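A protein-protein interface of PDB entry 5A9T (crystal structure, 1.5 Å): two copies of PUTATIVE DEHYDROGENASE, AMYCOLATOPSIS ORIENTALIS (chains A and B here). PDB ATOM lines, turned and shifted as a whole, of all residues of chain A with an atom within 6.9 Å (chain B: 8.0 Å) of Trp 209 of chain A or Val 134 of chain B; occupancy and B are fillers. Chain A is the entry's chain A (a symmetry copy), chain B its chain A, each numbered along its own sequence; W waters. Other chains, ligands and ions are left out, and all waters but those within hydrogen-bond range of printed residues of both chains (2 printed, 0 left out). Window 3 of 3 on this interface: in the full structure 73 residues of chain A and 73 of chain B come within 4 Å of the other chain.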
ATOM      1  N   THR A 203      -1.560 -11.767 -12.598  1.00  0.00           N
ATOM      2  CA  THR A 203      -2.454 -11.489 -13.757  1.00  0.00           C
ATOM      3  C   THR A 203      -2.732 -10.055 -14.129  1.00  0.00           C
ATOM      4  O   THR A 203      -3.030  -9.678 -15.243  1.00  0.00           O
ATOM      5  CB  THR A 203      -3.855 -12.153 -13.629  1.00  0.00           C
ATOM      6  OG1 THR A 203      -4.578 -11.419 -12.562  1.00  0.00           O
ATOM      7  CG2 THR A 203      -3.748 -13.559 -13.362  1.00  0.00           C
ATOM      8  N   LYS A 204      -2.633  -9.163 -13.122  1.00  0.00           N
ATOM      9  CA  LYS A 204      -2.764  -7.686 -13.387  1.00  0.00           C
ATOM     10  C   LYS A 204      -1.807  -7.205 -14.449  1.00  0.00           C
ATOM     11  O   LYS A 204      -2.197  -6.482 -15.376  1.00  0.00           O
ATOM     12  CB  LYS A 204      -2.549  -6.910 -12.079  1.00  0.00           C
ATOM     13  CG  LYS A 204      -3.618  -7.246 -11.046  1.00  0.00           C
ATOM     14  CD  LYS A 204      -3.334  -6.522  -9.716  1.00  0.00           C
ATOM     15  CE  LYS A 204      -4.390  -6.839  -8.728  1.00  0.00           C
ATOM     16  NZ  LYS A 204      -4.062  -6.085  -7.516  1.00  0.00           N
ATOM     17  N   LEU A 205      -0.562  -7.636 -14.399  1.00  0.00           N
ATOM     18  CA  LEU A 205       0.331  -7.275 -15.439  1.00  0.00           C
ATOM     19  C   LEU A 205       0.327  -8.318 -16.603  1.00  0.00           C
ATOM     20  O   LEU A 205       0.319  -7.940 -17.759  1.00  0.00           O
ATOM     21  CB  LEU A 205       1.741  -7.092 -14.916  1.00  0.00           C
ATOM     22  CG  LEU A 205       1.920  -5.768 -14.174  1.00  0.00           C
ATOM     23  CD1 LEU A 205       3.215  -5.800 -13.439  1.00  0.00           C
ATOM     24  CD2 LEU A 205       1.963  -4.605 -15.105  1.00  0.00           C
ATOM     25  N   ALA A 206       0.205  -9.584 -16.318  1.00  0.00           N
ATOM     26  CA  ALA A 206       0.375 -10.593 -17.353  1.00  0.00           C
ATOM     27  C   ALA A 206      -0.839 -10.657 -18.305  1.00  0.00           C
ATOM     28  O   ALA A 206      -0.620 -10.875 -19.505  1.00  0.00           O
ATOM     29  CB  ALA A 206       0.664 -11.958 -16.730  1.00  0.00           C
ATOM     30  N   VAL A 207      -2.042 -10.538 -17.768  1.00  0.00           N
ATOM     31  CA  VAL A 207      -3.262 -10.623 -18.561  1.00  0.00           C
ATOM     32  C   VAL A 207      -3.860  -9.305 -18.889  1.00  0.00           C
ATOM     33  O   VAL A 207      -4.242  -9.097 -20.050  1.00  0.00           O
ATOM     34  CB  VAL A 207      -4.309 -11.536 -17.809  1.00  0.00           C
ATOM     35  CG1 VAL A 207      -5.570 -11.534 -18.627  1.00  0.00           C
ATOM     36  CG2 VAL A 207      -3.703 -12.892 -17.680  1.00  0.00           C
ATOM     37  N   ASP A 208      -3.949  -8.382 -17.912  1.00  0.00           N
ATOM     38  CA  ASP A 208      -4.581  -7.148 -18.287  1.00  0.00           C
ATOM     39  C   ASP A 208      -3.794  -6.294 -19.207  1.00  0.00           C
ATOM     40  O   ASP A 208      -4.330  -5.475 -19.926  1.00  0.00           O
ATOM     41  CB  ASP A 208      -4.972  -6.381 -16.974  1.00  0.00           C
ATOM     42  CG  ASP A 208      -5.971  -7.125 -16.076  1.00  0.00           C
ATOM     43  OD1 ASP A 208      -6.729  -7.950 -16.588  1.00  0.00           O
ATOM     44  OD2 ASP A 208      -5.884  -6.948 -14.817  1.00  0.00           O
ATOM     45  N   TRP A 209      -2.450  -6.415 -19.179  1.00  0.00           N
ATOM     46  CA  TRP A 209      -1.562  -5.650 -19.999  1.00  0.00           C
ATOM     47  C   TRP A 209      -0.835  -6.526 -21.014  1.00  0.00           C
ATOM     48  O   TRP A 209      -1.005  -6.348 -22.213  1.00  0.00           O
ATOM     49  CB  TRP A 209      -0.568  -4.825 -19.116  1.00  0.00           C
ATOM     50  CG  TRP A 209       0.595  -4.337 -19.920  1.00  0.00           C
ATOM     51  CD1 TRP A 209       0.552  -3.481 -21.015  1.00  0.00           C
ATOM     52  CD2 TRP A 209       1.947  -4.699 -19.802  1.00  0.00           C
ATOM     53  NE1 TRP A 209       1.752  -3.360 -21.558  1.00  0.00           N
ATOM     54  CE2 TRP A 209       2.661  -4.080 -20.850  1.00  0.00           C
ATOM     55  CE3 TRP A 209       2.624  -5.513 -18.940  1.00  0.00           C
ATOM     56  CZ2 TRP A 209       4.007  -4.287 -21.024  1.00  0.00           C
ATOM     57  CZ3 TRP A 209       4.067  -5.640 -19.079  1.00  0.00           C
ATOM     58  CH2 TRP A 209       4.692  -5.010 -20.134  1.00  0.00           C
ATOM     59  N   PHE A 210       0.024  -7.441 -20.579  1.00  0.00           N
ATOM     60  CA  PHE A 210       1.013  -8.049 -21.483  1.00  0.00           C
ATOM     61  C   PHE A 210       0.375  -8.879 -22.571  1.00  0.00           C
ATOM     62  O   PHE A 210       0.760  -8.789 -23.763  1.00  0.00           O
ATOM     63  CB  PHE A 210       2.022  -8.844 -20.659  1.00  0.00           C
ATOM     64  CG  PHE A 210       3.249  -9.322 -21.402  1.00  0.00           C
ATOM     65  CD1 PHE A 210       4.332  -8.485 -21.587  1.00  0.00           C
ATOM     66  CD2 PHE A 210       3.324 -10.642 -21.871  1.00  0.00           C
ATOM     67  CE1 PHE A 210       5.431  -8.903 -22.261  1.00  0.00           C
ATOM     68  CE2 PHE A 210       4.441 -11.048 -22.536  1.00  0.00           C
ATOM     69  CZ  PHE A 210       5.474 -10.158 -22.744  1.00  0.00           C
ATOM     70  N   LEU A 211      -0.617  -9.697 -22.183  1.00  0.00           N
ATOM     71  CA  LEU A 211      -1.278 -10.533 -23.161  1.00  0.00           C
ATOM     72  C   LEU A 211      -1.819  -9.784 -24.387  1.00  0.00           C
ATOM     73  O   LEU A 211      -1.418 -10.086 -25.505  1.00  0.00           O
ATOM     74  CB  LEU A 211      -2.275 -11.438 -22.445  1.00  0.00           C
ATOM     75  CG  LEU A 211      -2.935 -12.527 -23.281  1.00  0.00           C
ATOM     76  CD1 LEU A 211      -1.975 -13.616 -23.710  1.00  0.00           C
ATOM     77  CD2 LEU A 211      -4.071 -13.082 -22.496  1.00  0.00           C
ATOM     78  N   PRO A 212      -2.672  -8.780 -24.196  1.00  0.00           N
ATOM     79  CA  PRO A 212      -3.148  -8.083 -25.359  1.00  0.00           C
ATOM     80  C   PRO A 212      -2.202  -7.055 -25.934  1.00  0.00           C
ATOM     81  O   PRO A 212      -2.058  -6.957 -27.182  1.00  0.00           O
ATOM     82  CB  PRO A 212      -4.410  -7.414 -24.811  1.00  0.00           C
ATOM     83  CG  PRO A 212      -4.174  -7.258 -23.338  1.00  0.00           C
ATOM     84  CD  PRO A 212      -3.422  -8.474 -22.979  1.00  0.00           C
ATOM     85  N   ALA A 213      -1.506  -6.298 -25.064  1.00  0.00           N
ATOM     86  CA  ALA A 213      -0.748  -5.177 -25.529  1.00  0.00           C
ATOM     87  C   ALA A 213       0.558  -5.496 -26.114  1.00  0.00           C
ATOM     88  O   ALA A 213       1.147  -4.691 -26.864  1.00  0.00           O
ATOM     89  CB  ALA A 213      -0.626  -4.131 -24.423  1.00  0.00           C
ATOM     90  N   VAL A 214       1.171  -6.611 -25.686  1.00  0.00           N
ATOM     91  CA  VAL A 214       2.413  -7.040 -26.184  1.00  0.00           C
ATOM     92  C   VAL A 214       2.218  -8.265 -27.076  1.00  0.00           C
ATOM     93  O   VAL A 214       2.546  -8.227 -28.244  1.00  0.00           O
ATOM     94  CB  VAL A 214       3.496  -7.269 -25.068  1.00  0.00           C
ATOM     95  CG1 VAL A 214       4.795  -7.735 -25.689  1.00  0.00           C
ATOM     96  CG2 VAL A 214       3.676  -5.983 -24.235  1.00  0.00           C
ATOM     97  N   ILE A 215       1.806  -9.404 -26.536  1.00  0.00           N
ATOM     98  CA  ILE A 215       1.718 -10.630 -27.354  1.00  0.00           C
ATOM     99  C   ILE A 215       0.780 -10.379 -28.535  1.00  0.00           C
ATOM    100  O   ILE A 215       1.117 -10.647 -29.698  1.00  0.00           O
ATOM    101  CB  ILE A 215       1.290 -11.802 -26.439  1.00  0.00           C
ATOM    102  CG1 ILE A 215       2.390 -12.103 -25.376  1.00  0.00           C
ATOM    103  CG2 ILE A 215       1.108 -13.040 -27.345  1.00  0.00           C
ATOM    104  CD1 ILE A 215       1.998 -13.121 -24.348  1.00  0.00           C
ATOM    105  N   ALA B 120      13.499  -3.248 -15.813  1.00  0.00           N
ATOM    106  CA  ALA B 120      13.427  -4.101 -16.987  1.00  0.00           C
ATOM    107  C   ALA B 120      12.626  -3.394 -18.075  1.00  0.00           C
ATOM    108  O   ALA B 120      11.459  -2.990 -17.865  1.00  0.00           O
ATOM    109  CB  ALA B 120      12.760  -5.447 -16.628  1.00  0.00           C
ATOM    110  N   ILE B 121      13.231  -3.218 -19.224  1.00  0.00           N
ATOM    111  CA  ILE B 121      12.616  -2.506 -20.341  1.00  0.00           C
ATOM    112  C   ILE B 121      11.800  -3.488 -21.178  1.00  0.00           C
ATOM    113  O   ILE B 121      12.332  -4.476 -21.636  1.00  0.00           O
ATOM    114  CB  ILE B 121      13.705  -1.888 -21.182  1.00  0.00           C
ATOM    115  CG1 ILE B 121      14.556  -0.929 -20.318  1.00  0.00           C
ATOM    116  CG2 ILE B 121      13.059  -1.167 -22.337  1.00  0.00           C
ATOM    117  CD1 ILE B 121      15.825  -0.456 -21.019  1.00  0.00           C
ATOM    118  N   MET B 122      10.508  -3.220 -21.312  1.00  0.00           N
ATOM    119  CA  MET B 122       9.584  -4.207 -21.922  1.00  0.00           C
ATOM    120  C   MET B 122       9.303  -3.958 -23.354  1.00  0.00           C
ATOM    121  O   MET B 122       8.391  -4.600 -23.853  1.00  0.00           O
ATOM    122  CB  MET B 122       8.343  -4.283 -21.093  1.00  0.00           C
ATOM    123  CG  MET B 122       8.576  -4.653 -19.646  1.00  0.00           C
ATOM    124  SD  MET B 122       9.522  -6.152 -19.356  1.00  0.00           S
ATOM    125  CE  MET B 122       8.429  -7.410 -20.072  1.00  0.00           C
ATOM    126  N   VAL B 123      10.060  -3.144 -24.010  1.00  0.00           N
ATOM    127  CA  VAL B 123       9.832  -2.785 -25.424  1.00  0.00           C
ATOM    128  C   VAL B 123      11.149  -2.670 -26.098  1.00  0.00           C
ATOM    129  O   VAL B 123      12.228  -2.564 -25.489  1.00  0.00           O
ATOM    130  CB  VAL B 123       8.980  -1.474 -25.588  1.00  0.00           C
ATOM    131  CG1 VAL B 123       7.656  -1.686 -24.973  1.00  0.00           C
ATOM    132  CG2 VAL B 123       9.783  -0.299 -24.967  1.00  0.00           C
ATOM    133  N   PRO B 124      11.193  -2.698 -27.414  1.00  0.00           N
ATOM    134  CA  PRO B 124      12.459  -2.473 -28.083  1.00  0.00           C
ATOM    135  C   PRO B 124      12.901  -1.016 -28.059  1.00  0.00           C
ATOM    136  O   PRO B 124      12.083  -0.091 -27.796  1.00  0.00           O
ATOM    137  CB  PRO B 124      12.208  -2.973 -29.578  1.00  0.00           C
ATOM    138  CG  PRO B 124      10.779  -3.387 -29.539  1.00  0.00           C
ATOM    139  CD  PRO B 124      10.085  -3.115 -28.295  1.00  0.00           C
ATOM    140  N   MET B 127      10.832   1.906 -29.412  1.00  0.00           N
ATOM    141  CA  MET B 127       9.653   2.275 -28.742  1.00  0.00           C
ATOM    142  C   MET B 127       9.832   3.093 -27.395  1.00  0.00           C
ATOM    143  O   MET B 127       8.901   3.648 -26.825  1.00  0.00           O
ATOM    144  CB  MET B 127       8.793   1.070 -28.451  1.00  0.00           C
ATOM    145  CG  MET B 127       8.173   0.555 -29.743  1.00  0.00           C
ATOM    146  SD  MET B 127       7.013  -0.724 -29.319  1.00  0.00           S
ATOM    147  CE  MET B 127       6.003   0.018 -28.031  1.00  0.00           C
ATOM    148  N   VAL B 128      11.115   3.153 -26.979  1.00  0.00           N
ATOM    149  CA  VAL B 128      11.419   3.898 -25.768  1.00  0.00           C
ATOM    150  C   VAL B 128      10.985   5.344 -25.935  1.00  0.00           C
ATOM    151  O   VAL B 128      11.211   5.958 -27.018  1.00  0.00           O
ATOM    152  CB  VAL B 128      12.934   3.784 -25.403  1.00  0.00           C
ATOM    153  CG1 VAL B 128      13.248   4.803 -24.272  1.00  0.00           C
ATOM    154  CG2 VAL B 128      13.266   2.253 -25.096  1.00  0.00           C
ATOM    155  N   GLY B 129      10.285   5.903 -24.961  1.00  0.00           N
ATOM    156  CA  GLY B 129       9.757   7.263 -24.975  1.00  0.00           C
ATOM    157  C   GLY B 129       8.441   7.471 -25.674  1.00  0.00           C
ATOM    158  O   GLY B 129       7.971   8.611 -25.712  1.00  0.00           O
ATOM    159  N   HIS B 130       7.903   6.416 -26.278  1.00  0.00           N
ATOM    160  CA  HIS B 130       6.634   6.426 -27.040  1.00  0.00           C
ATOM    161  C   HIS B 130       5.518   5.783 -26.322  1.00  0.00           C
ATOM    162  O   HIS B 130       5.717   5.020 -25.343  1.00  0.00           O
ATOM    163  CB  HIS B 130       6.852   5.843 -28.425  1.00  0.00           C
ATOM    164  CG  HIS B 130       7.851   6.617 -29.250  1.00  0.00           C
ATOM    165  ND1 HIS B 130       7.576   7.863 -29.803  1.00  0.00           N
ATOM    166  CD2 HIS B 130       9.120   6.323 -29.621  1.00  0.00           C
ATOM    167  CE1 HIS B 130       8.659   8.321 -30.414  1.00  0.00           C
ATOM    168  NE2 HIS B 130       9.604   7.400 -30.334  1.00  0.00           N
ATOM    169  N   PRO B 131       4.259   6.131 -26.686  1.00  0.00           N
ATOM    170  CA  PRO B 131       3.101   5.503 -26.022  1.00  0.00           C
ATOM    171  C   PRO B 131       3.181   3.988 -26.222  1.00  0.00           C
ATOM    172  O   PRO B 131       3.612   3.493 -27.284  1.00  0.00           O
ATOM    173  CB  PRO B 131       1.892   6.090 -26.836  1.00  0.00           C
ATOM    174  CG  PRO B 131       2.417   7.418 -27.261  1.00  0.00           C
ATOM    175  CD  PRO B 131       3.842   7.138 -27.697  1.00  0.00           C
ATOM    176  N   GLY B 132       2.976   3.250 -25.162  1.00  0.00           N
ATOM    177  CA  GLY B 132       3.145   1.780 -25.275  1.00  0.00           C
ATOM    178  C   GLY B 132       4.348   1.296 -24.454  1.00  0.00           C
ATOM    179  O   GLY B 132       4.421   0.104 -24.000  1.00  0.00           O
ATOM    180  N   SER B 133       5.326   2.157 -24.284  1.00  0.00           N
ATOM    181  CA  SER B 133       6.500   1.715 -23.613  1.00  0.00           C
ATOM    182  C   SER B 133       6.234   1.602 -22.135  1.00  0.00           C
ATOM    183  O   SER B 133       5.499   2.416 -21.551  1.00  0.00           O
ATOM    184  CB  SER B 133       7.582   2.723 -23.837  1.00  0.00           C
ATOM    185  OG  SER B 133       8.778   2.437 -23.053  1.00  0.00           O
ATOM    186  N   VAL B 134       6.665   0.461 -21.576  1.00  0.00           N
ATOM    187  CA  VAL B 134       6.473   0.092 -20.148  1.00  0.00           C
ATOM    188  C   VAL B 134       7.817  -0.326 -19.646  1.00  0.00           C
ATOM    189  O   VAL B 134       8.509  -1.117 -20.278  1.00  0.00           O
ATOM    190  CB  VAL B 134       5.462  -1.066 -19.949  1.00  0.00           C
ATOM    191  CG1 VAL B 134       5.390  -1.540 -18.526  1.00  0.00           C
ATOM    192  CG2 VAL B 134       4.119  -0.553 -20.420  1.00  0.00           C
ATOM    193  N   PHE B 135       8.186   0.182 -18.477  1.00  0.00           N
ATOM    194  CA  PHE B 135       9.408  -0.242 -17.771  1.00  0.00           C
ATOM    195  C   PHE B 135       9.007  -0.705 -16.394  1.00  0.00           C
ATOM    196  O   PHE B 135       8.210  -0.028 -15.708  1.00  0.00           O
ATOM    197  CB  PHE B 135      10.370   0.946 -17.579  1.00  0.00           C
ATOM    198  CG  PHE B 135      11.176   1.415 -18.773  1.00  0.00           C
ATOM    199  CD1 PHE B 135      10.656   1.495 -20.054  1.00  0.00           C
ATOM    200  CD2 PHE B 135      12.431   1.868 -18.592  1.00  0.00           C
ATOM    201  CE1 PHE B 135      11.391   1.922 -21.144  1.00  0.00           C
ATOM    202  CE2 PHE B 135      13.142   2.256 -19.704  1.00  0.00           C
ATOM    203  CZ  PHE B 135      12.634   2.327 -20.956  1.00  0.00           C
ATOM    204  N   LEU B 136       9.436  -1.915 -16.014  1.00  0.00           N
ATOM    205  CA  LEU B 136       9.156  -2.483 -14.704  1.00  0.00           C
ATOM    206  C   LEU B 136      10.347  -2.220 -13.759  1.00  0.00           C
ATOM    207  O   LEU B 136      11.488  -2.392 -14.192  1.00  0.00           O
ATOM    208  CB  LEU B 136       8.905  -3.969 -14.757  1.00  0.00           C
ATOM    209  CG  LEU B 136       7.819  -4.391 -15.774  1.00  0.00           C
ATOM    210  CD1 LEU B 136       7.692  -5.910 -15.732  1.00  0.00           C
ATOM    211  CD2 LEU B 136       6.479  -3.763 -15.506  1.00  0.00           C
ATOM    212  N   TYR B 137      10.087  -1.743 -12.573  1.00  0.00           N
ATOM    213  CA  TYR B 137      11.110  -1.422 -11.619  1.00  0.00           C
ATOM    214  C   TYR B 137      10.961  -2.165 -10.280  1.00  0.00           C
ATOM    215  O   TYR B 137       9.873  -2.458  -9.825  1.00  0.00           O
ATOM    216  CB  TYR B 137      11.134   0.086 -11.320  1.00  0.00           C
ATOM    217  CG  TYR B 137      11.454   0.961 -12.480  1.00  0.00           C
ATOM    218  CD1 TYR B 137      12.730   1.271 -12.837  1.00  0.00           C
ATOM    219  CD2 TYR B 137      10.433   1.516 -13.305  1.00  0.00           C
ATOM    220  CE1 TYR B 137      13.022   2.035 -13.945  1.00  0.00           C
ATOM    221  CE2 TYR B 137      10.702   2.299 -14.361  1.00  0.00           C
ATOM    222  CZ  TYR B 137      11.995   2.578 -14.702  1.00  0.00           C
ATOM    223  OH  TYR B 137      12.328   3.366 -15.756  1.00  0.00           O
ATOM    224  N   LEU B 154      10.651   7.788 -20.295  1.00  0.00           N
ATOM    225  CA  LEU B 154      11.158   6.670 -20.982  1.00  0.00           C
ATOM    226  C   LEU B 154      10.007   5.678 -21.339  1.00  0.00           C
ATOM    227  O   LEU B 154      10.097   4.927 -22.338  1.00  0.00           O
ATOM    228  CB  LEU B 154      12.191   5.939 -20.144  1.00  0.00           C
ATOM    229  CG  LEU B 154      13.398   6.808 -19.666  1.00  0.00           C
ATOM    230  CD1 LEU B 154      14.313   6.043 -18.750  1.00  0.00           C
ATOM    231  CD2 LEU B 154      14.186   7.310 -20.858  1.00  0.00           C
ATOM    232  N   GLY B 155       9.074   5.558 -20.448  1.00  0.00           N
ATOM    233  CA  GLY B 155       7.966   4.584 -20.567  1.00  0.00           C
ATOM    234  C   GLY B 155       7.170   4.608 -19.301  1.00  0.00           C
ATOM    235  O   GLY B 155       7.599   5.149 -18.253  1.00  0.00           O
ATOM    236  N   ASP B 156       5.970   4.054 -19.274  1.00  0.00           N
ATOM    237  CA  ASP B 156       5.160   3.989 -18.145  1.00  0.00           C
ATOM    238  C   ASP B 156       5.879   3.243 -17.025  1.00  0.00           C
ATOM    239  O   ASP B 156       6.153   2.065 -17.195  1.00  0.00           O
ATOM    240  CB  ASP B 156       3.831   3.252 -18.394  1.00  0.00           C
ATOM    241  CG  ASP B 156       2.877   3.349 -17.241  1.00  0.00           C
ATOM    242  OD1 ASP B 156       2.927   4.327 -16.477  1.00  0.00           O
ATOM    243  OD2 ASP B 156       1.975   2.446 -17.104  1.00  0.00           O
ATOM    244  N   PRO B 157       6.140   3.867 -15.871  1.00  0.00           N
ATOM    245  CA  PRO B 157       6.960   3.218 -14.889  1.00  0.00           C
ATOM    246  C   PRO B 157       6.082   2.465 -13.878  1.00  0.00           C
ATOM    247  O   PRO B 157       5.135   3.026 -13.332  1.00  0.00           O
ATOM    248  CB  PRO B 157       7.665   4.381 -14.224  1.00  0.00           C
ATOM    249  CG  PRO B 157       6.725   5.509 -14.334  1.00  0.00           C
ATOM    250  CD  PRO B 157       5.963   5.312 -15.589  1.00  0.00           C
ATOM    251  N   VAL B 158       6.363   1.207 -13.605  1.00  0.00           N
ATOM    252  CA  VAL B 158       5.663   0.344 -12.679  1.00  0.00           C
ATOM    253  C   VAL B 158       6.609  -0.155 -11.617  1.00  0.00           C
ATOM    254  O   VAL B 158       7.596  -0.762 -11.898  1.00  0.00           O
ATOM    255  CB  VAL B 158       5.046  -0.888 -13.402  1.00  0.00           C
ATOM    256  CG1 VAL B 158       4.359  -1.751 -12.369  1.00  0.00           C
ATOM    257  CG2 VAL B 158       4.044  -0.440 -14.426  1.00  0.00           C
ATOM    258  N   TYR B 170      10.166 -10.745 -13.274  1.00  0.00           N
ATOM    259  CA  TYR B 170       8.962 -10.543 -14.070  1.00  0.00           C
ATOM    260  C   TYR B 170       9.230 -10.575 -15.512  1.00  0.00           C
ATOM    261  O   TYR B 170       8.481 -11.143 -16.350  1.00  0.00           O
ATOM    262  CB  TYR B 170       8.288  -9.203 -13.697  1.00  0.00           C
ATOM    263  CG  TYR B 170       7.127  -9.253 -12.719  1.00  0.00           C
ATOM    264  CD1 TYR B 170       7.307  -9.467 -11.382  1.00  0.00           C
ATOM    265  CD2 TYR B 170       5.868  -9.093 -13.227  1.00  0.00           C
ATOM    266  CE1 TYR B 170       6.094  -9.441 -10.527  1.00  0.00           C
ATOM    267  CE2 TYR B 170       4.757  -9.099 -12.431  1.00  0.00           C
ATOM    268  CZ  TYR B 170       4.920  -9.236 -11.137  1.00  0.00           C
ATOM    269  OH  TYR B 170       3.586  -9.266 -10.501  1.00  0.00           O
ATOM    270  N   ASN B 171      10.305  -9.906 -15.979  1.00  0.00           N
ATOM    271  CA  ASN B 171      10.678  -9.906 -17.383  1.00  0.00           C
ATOM    272  C   ASN B 171      10.875 -11.359 -17.880  1.00  0.00           C
ATOM    273  O   ASN B 171      10.339 -11.722 -18.907  1.00  0.00           O
ATOM    274  CB  ASN B 171      11.924  -9.092 -17.634  1.00  0.00           C
ATOM    275  CG  ASN B 171      12.176  -8.869 -19.098  1.00  0.00           C
ATOM    276  OD1 ASN B 171      11.326  -8.804 -19.941  1.00  0.00           O
ATOM    277  ND2 ASN B 171      13.390  -8.794 -19.408  1.00  0.00           N
ATOM    278  N   LEU B 174       7.472 -13.080 -18.083  1.00  0.00           N
ATOM    279  CA  LEU B 174       6.629 -12.653 -19.179  1.00  0.00           C
ATOM    280  C   LEU B 174       7.204 -13.151 -20.518  1.00  0.00           C
ATOM    281  O   LEU B 174       6.434 -13.505 -21.419  1.00  0.00           O
ATOM    282  CB  LEU B 174       6.431 -11.135 -19.128  1.00  0.00           C
ATOM    283  CG  LEU B 174       5.633 -10.590 -17.924  1.00  0.00           C
ATOM    284  CD1 LEU B 174       5.804  -9.101 -17.754  1.00  0.00           C
ATOM    285  CD2 LEU B 174       4.124 -11.012 -18.018  1.00  0.00           C
ATOM    286  N   MET B 177       6.267 -16.763 -20.965  1.00  0.00           N
ATOM    287  CA  MET B 177       4.877 -16.823 -21.382  1.00  0.00           C
ATOM    288  C   MET B 177       4.763 -16.447 -22.865  1.00  0.00           C
ATOM    289  O   MET B 177       3.959 -17.103 -23.614  1.00  0.00           O
ATOM    290  CB  MET B 177       4.040 -15.903 -20.532  1.00  0.00           C
ATOM    291  CG  MET B 177       2.595 -15.820 -21.009  1.00  0.00           C
ATOM    292  SD  MET B 177       1.702 -14.720 -19.816  1.00  0.00           S
ATOM    293  CE  MET B 177       0.221 -14.136 -20.654  1.00  0.00           C
HETATM  294  O   HOH W   1       1.105  -7.905 -11.558  1.00  0.00           O
HETATM  295  O   HOH W   2       2.264  -1.583 -23.855  1.00  0.00           O
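Tyr 170 of chain B touches Leu 205 of chain A. Leu 174 of chain B touches Ala 206 of chain A. Met 177 of chain B touches Ala 206 of chain A. Trp 209 of chain A touches Met 122 of chain B. Trp 209 of chain A touches Val 134 of chain B. Phe 210 of chain A touches Leu 174 of chain B (CE2 to O, 3.4 Å). Leu 211 of chain A touches Met 177 of chain B.
Water W2 lies within hydrogen-bond range of O of Gly 132 of chain B and NE1 of Trp 209 of chain A. Water W1 bridges the side-chain hydroxyl (OH) of Tyr 170 of chain B (3.0 Å) and the backbone NH (N) of Leu 205 of chain A (3.3 Å).
No position is printed for both chains. Of the 7 pairs that touch across the chains among the printed residues, none has its exchanged pair printed and touching as well.
Of the 25 printed residues of chain B, 5 touch a printed residue of chain A. Hydrophobic or aromatic side chains of chain B that line the printed part of chain A: Met 122, Val 134, Tyr 170, Leu 174 and Met 177. Printed residues of chain A that touch a printed residue of chain B: Leu 205, Ala 206, Trp 209, Phe 210 and Leu 211. Hydrophobic or aromatic side chains of chain A within 4 Å of the printed part of chain B: Leu 205, Ala 206, Trp 209, Phe 210 and Leu 211.
Of chain B, only Met 122 and Val 134 come within 4 Å of Trp 209 of chain A. Of the printed residues of chain B, Leu 211 of chain A touches Met 177 (3.8 Å). Ser 133 of chain B touches none of the printed residues of chain A. Val 134 of chain B touches one residue of chain A. Val 158 of chain B touches none of the printed residues of chain A. Printed residues of chain A within 4 Å of Tyr 170 of chain B: Leu 205. Of the printed residues of chain A, Leu 174 of chain B touches Ala 206 and Phe 210. The nearest residue of chain B that does not touch Trp 209 of chain A is Leu 174 of chain B (4.1 Å). The nearest residue of chain A that does not touch Val 134 of chain B is Leu 205 of chain A (5.7 Å).
O of Val 134 of chain B lies within hydrogen-bond range of N of Met 122 of chain B (3.1 Å). The side-chain sulfur (SD) of Met 122 of chain B sits close to the side-chain amide oxygen (OD1) of Asn 171 of chain B (3.3 Å). N of Phe 210 of chain A lies within hydrogen-bond range of O of Leu 205 of chain A (2.9 Å). The backbone carbonyl oxygen (O) of Ala 206 of chain A is in hydrogen-bond range of the backbone NH (N) of Leu 211 of chain A. O of Phe 210 of chain A sits at hydrogen-bond distance from N of Ile 215 of chain A.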
